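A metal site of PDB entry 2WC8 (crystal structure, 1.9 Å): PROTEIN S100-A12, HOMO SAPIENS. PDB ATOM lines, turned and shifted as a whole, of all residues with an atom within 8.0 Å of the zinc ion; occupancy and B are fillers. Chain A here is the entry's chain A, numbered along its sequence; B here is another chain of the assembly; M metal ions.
NE2 of His 93 of chain B lies close to OG1 of Thr 92 of chain B, at 3.5 Å.
O of His 19 lies close to OG of Ser 22, 3.4 Å away.
O of His 89 of chain B sits at hydrogen-bond distance from OG1 of Thr 92 of chain B (2.8 Å).
The zinc ion is bound by OD1 of Asp 29 (1.9 Å), NE2 of His 93 of chain B (2.0 Å), NE2 of His 19 (2.1 Å) and NE2 of His 89 of chain B (2.1 Å).
The zinc ion has four donor atoms within binding distance.
Slightly farther from the zinc ion lies OD2 of Asp 29 (2.8 Å).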
ATOM      1  N   VAL A  15     -32.507 -16.640  10.619  1.00  0.00           N
ATOM      2  CA  VAL A  15     -31.423 -17.577  10.426  1.00  0.00           C
ATOM      3  C   VAL A  15     -30.227 -17.231  11.340  1.00  0.00           C
ATOM      4  O   VAL A  15     -29.641 -18.134  11.943  1.00  0.00           O
ATOM      5  CB  VAL A  15     -30.956 -17.650   8.945  1.00  0.00           C
ATOM      6  CG1 VAL A  15     -29.723 -18.585   8.841  1.00  0.00           C
ATOM      7  CG2 VAL A  15     -32.114 -18.144   7.981  1.00  0.00           C
ATOM      8  N   PHE A  18     -30.919 -18.297  15.032  1.00  0.00           N
ATOM      9  CA  PHE A  18     -30.755 -19.725  15.097  1.00  0.00           C
ATOM     10  C   PHE A  18     -29.288 -20.072  15.226  1.00  0.00           C
ATOM     11  O   PHE A  18     -28.892 -20.857  16.065  1.00  0.00           O
ATOM     12  CB  PHE A  18     -31.347 -20.429  13.863  1.00  0.00           C
ATOM     13  CG  PHE A  18     -31.119 -21.881  13.868  1.00  0.00           C
ATOM     14  CD1 PHE A  18     -31.954 -22.703  14.633  1.00  0.00           C
ATOM     15  CD2 PHE A  18     -30.072 -22.434  13.160  1.00  0.00           C
ATOM     16  CE1 PHE A  18     -31.740 -24.124  14.669  1.00  0.00           C
ATOM     17  CE2 PHE A  18     -29.830 -23.864  13.218  1.00  0.00           C
ATOM     18  CZ  PHE A  18     -30.686 -24.696  13.948  1.00  0.00           C
ATOM     19  N   HIS A  19     -28.493 -19.515  14.343  1.00  0.00           N
ATOM     20  CA  HIS A  19     -27.079 -19.874  14.321  1.00  0.00           C
ATOM     21  C   HIS A  19     -26.318 -19.458  15.576  1.00  0.00           C
ATOM     22  O   HIS A  19     -25.406 -20.153  16.006  1.00  0.00           O
ATOM     23  CB  HIS A  19     -26.474 -19.242  13.075  1.00  0.00           C
ATOM     24  CG  HIS A  19     -26.697 -20.030  11.842  1.00  0.00           C
ATOM     25  ND1 HIS A  19     -26.693 -19.462  10.579  1.00  0.00           N
ATOM     26  CD2 HIS A  19     -26.807 -21.375  11.656  1.00  0.00           C
ATOM     27  CE1 HIS A  19     -26.794 -20.421   9.669  1.00  0.00           C
ATOM     28  NE2 HIS A  19     -26.873 -21.588  10.297  1.00  0.00           N
ATOM     29  N   SER A  22     -27.152 -22.330  17.778  1.00  0.00           N
ATOM     30  CA  SER A  22     -26.704 -23.584  17.201  1.00  0.00           C
ATOM     31  C   SER A  22     -25.174 -23.709  17.174  1.00  0.00           C
ATOM     32  O   SER A  22     -24.632 -24.818  17.373  1.00  0.00           O
ATOM     33  CB  SER A  22     -27.308 -23.829  15.780  1.00  0.00           C
ATOM     34  OG  SER A  22     -26.796 -22.994  14.750  1.00  0.00           O
ATOM     35  N   HIS A  27     -22.322 -29.829  17.016  1.00  0.00           N
ATOM     36  CA  HIS A  27     -22.388 -29.410  15.630  1.00  0.00           C
ATOM     37  C   HIS A  27     -23.004 -28.053  15.511  1.00  0.00           C
ATOM     38  O   HIS A  27     -23.961 -27.793  16.201  1.00  0.00           O
ATOM     39  CB  HIS A  27     -23.125 -30.373  14.708  1.00  0.00           C
ATOM     40  CG  HIS A  27     -22.944 -29.967  13.271  1.00  0.00           C
ATOM     41  ND1 HIS A  27     -21.708 -30.021  12.634  1.00  0.00           N
ATOM     42  CD2 HIS A  27     -23.804 -29.393  12.399  1.00  0.00           C
ATOM     43  CE1 HIS A  27     -21.843 -29.539  11.409  1.00  0.00           C
ATOM     44  NE2 HIS A  27     -23.098 -29.137  11.245  1.00  0.00           N
ATOM     45  N   PHE A  28     -22.390 -27.212  14.675  1.00  0.00           N
ATOM     46  CA  PHE A  28     -22.804 -25.826  14.479  1.00  0.00           C
ATOM     47  C   PHE A  28     -24.232 -25.582  13.898  1.00  0.00           C
ATOM     48  O   PHE A  28     -24.741 -24.481  13.987  1.00  0.00           O
ATOM     49  CB  PHE A  28     -21.764 -25.034  13.657  1.00  0.00           C
ATOM     50  CG  PHE A  28     -21.688 -25.417  12.170  1.00  0.00           C
ATOM     51  CD1 PHE A  28     -22.765 -25.265  11.312  1.00  0.00           C
ATOM     52  CD2 PHE A  28     -20.504 -25.947  11.622  1.00  0.00           C
ATOM     53  CE1 PHE A  28     -22.645 -25.621   9.942  1.00  0.00           C
ATOM     54  CE2 PHE A  28     -20.420 -26.291  10.253  1.00  0.00           C
ATOM     55  CZ  PHE A  28     -21.497 -26.143   9.447  1.00  0.00           C
ATOM     56  N   ASP A  29     -24.837 -26.594  13.289  1.00  0.00           N
ATOM     57  CA  ASP A  29     -26.131 -26.414  12.656  1.00  0.00           C
ATOM     58  C   ASP A  29     -27.308 -27.091  13.348  1.00  0.00           C
ATOM     59  O   ASP A  29     -28.441 -27.102  12.817  1.00  0.00           O
ATOM     60  CB  ASP A  29     -26.038 -26.888  11.192  1.00  0.00           C
ATOM     61  CG  ASP A  29     -26.478 -25.814  10.232  1.00  0.00           C
ATOM     62  OD1 ASP A  29     -26.524 -24.619  10.620  1.00  0.00           O
ATOM     63  OD2 ASP A  29     -26.779 -26.133   9.074  1.00  0.00           O
ATOM     64  N   THR A  30     -27.052 -27.692  14.489  1.00  0.00           N
ATOM     65  CA  THR A  30     -28.147 -28.225  15.275  1.00  0.00           C
ATOM     66  C   THR A  30     -28.083 -27.813  16.726  1.00  0.00           C
ATOM     67  O   THR A  30     -27.059 -27.327  17.228  1.00  0.00           O
ATOM     68  CB  THR A  30     -28.267 -29.743  15.114  1.00  0.00           C
ATOM     69  OG1 THR A  30     -27.128 -30.367  15.666  1.00  0.00           O
ATOM     70  CG2 THR A  30     -28.374 -30.099  13.661  1.00  0.00           C
ATOM     71  N   PHE A  74     -32.585 -27.036  11.629  1.00  0.00           N
ATOM     72  CA  PHE A  74     -33.253 -25.804  11.180  1.00  0.00           C
ATOM     73  C   PHE A  74     -34.685 -26.072  10.668  1.00  0.00           C
ATOM     74  O   PHE A  74     -35.622 -25.309  10.953  1.00  0.00           O
ATOM     75  CB  PHE A  74     -32.443 -25.075  10.097  1.00  0.00           C
ATOM     76  CG  PHE A  74     -32.914 -23.672   9.874  1.00  0.00           C
ATOM     77  CD1 PHE A  74     -32.727 -22.708  10.863  1.00  0.00           C
ATOM     78  CD2 PHE A  74     -33.674 -23.344   8.755  1.00  0.00           C
ATOM     79  CE1 PHE A  74     -33.200 -21.453  10.724  1.00  0.00           C
ATOM     80  CE2 PHE A  74     -34.169 -22.045   8.612  1.00  0.00           C
ATOM     81  CZ  PHE A  74     -33.918 -21.098   9.588  1.00  0.00           C
ATOM     82  N   ALA B  88     -33.232 -19.250   2.482  1.00  0.00           N
ATOM     83  CA  ALA B  88     -32.343 -18.277   3.148  1.00  0.00           C
ATOM     84  C   ALA B  88     -31.268 -18.985   4.003  1.00  0.00           C
ATOM     85  O   ALA B  88     -30.081 -18.645   3.962  1.00  0.00           O
ATOM     86  CB  ALA B  88     -33.106 -17.329   3.967  1.00  0.00           C
ATOM     87  N   HIS B  89     -31.668 -20.034   4.684  1.00  0.00           N
ATOM     88  CA  HIS B  89     -30.692 -20.805   5.461  1.00  0.00           C
ATOM     89  C   HIS B  89     -29.728 -21.587   4.596  1.00  0.00           C
ATOM     90  O   HIS B  89     -28.495 -21.526   4.805  1.00  0.00           O
ATOM     91  CB  HIS B  89     -31.422 -21.765   6.396  1.00  0.00           C
ATOM     92  CG  HIS B  89     -30.487 -22.635   7.186  1.00  0.00           C
ATOM     93  ND1 HIS B  89     -30.448 -24.000   7.037  1.00  0.00           N
ATOM     94  CD2 HIS B  89     -29.531 -22.326   8.090  1.00  0.00           C
ATOM     95  CE1 HIS B  89     -29.513 -24.498   7.820  1.00  0.00           C
ATOM     96  NE2 HIS B  89     -28.936 -23.514   8.463  1.00  0.00           N
ATOM     97  N   TYR B  90     -30.239 -22.282   3.581  1.00  0.00           N
ATOM     98  CA  TYR B  90     -29.389 -23.033   2.697  1.00  0.00           C
ATOM     99  C   TYR B  90     -28.357 -22.108   2.050  1.00  0.00           C
ATOM    100  O   TYR B  90     -27.186 -22.455   1.854  1.00  0.00           O
ATOM    101  CB  TYR B  90     -30.255 -23.716   1.642  1.00  0.00           C
ATOM    102  CG  TYR B  90     -29.534 -24.492   0.591  1.00  0.00           C
ATOM    103  CD1 TYR B  90     -29.101 -25.801   0.815  1.00  0.00           C
ATOM    104  CD2 TYR B  90     -29.289 -23.913  -0.647  1.00  0.00           C
ATOM    105  CE1 TYR B  90     -28.458 -26.506  -0.157  1.00  0.00           C
ATOM    106  CE2 TYR B  90     -28.640 -24.612  -1.629  1.00  0.00           C
ATOM    107  CZ  TYR B  90     -28.214 -25.909  -1.404  1.00  0.00           C
ATOM    108  OH  TYR B  90     -27.580 -26.589  -2.449  1.00  0.00           O
ATOM    109  N   THR B  92     -26.835 -19.483   3.275  1.00  0.00           N
ATOM    110  CA  THR B  92     -25.760 -19.125   4.157  1.00  0.00           C
ATOM    111  C   THR B  92     -24.687 -20.181   4.037  1.00  0.00           C
ATOM    112  O   THR B  92     -23.530 -19.876   4.244  1.00  0.00           O
ATOM    113  CB  THR B  92     -26.171 -18.972   5.688  1.00  0.00           C
ATOM    114  OG1 THR B  92     -26.497 -20.258   6.250  1.00  0.00           O
ATOM    115  CG2 THR B  92     -27.333 -18.032   5.871  1.00  0.00           C
ATOM    116  N   HIS B  93     -25.035 -21.434   3.670  1.00  0.00           N
ATOM    117  CA  HIS B  93     -24.005 -22.442   3.537  1.00  0.00           C
ATOM    118  C   HIS B  93     -23.541 -22.734   2.101  1.00  0.00           C
ATOM    119  O   HIS B  93     -22.832 -23.664   1.879  1.00  0.00           O
ATOM    120  CB  HIS B  93     -24.421 -23.734   4.244  1.00  0.00           C
ATOM    121  CG  HIS B  93     -24.741 -23.538   5.690  1.00  0.00           C
ATOM    122  ND1 HIS B  93     -23.801 -23.156   6.616  1.00  0.00           N
ATOM    123  CD2 HIS B  93     -25.932 -23.607   6.354  1.00  0.00           C
ATOM    124  CE1 HIS B  93     -24.379 -23.023   7.801  1.00  0.00           C
ATOM    125  NE2 HIS B  93     -25.670 -23.307   7.674  1.00  0.00           N
HETATM  126 ZN    ZN M   1     -26.954 -23.351   9.214  1.00  0.00          ZN
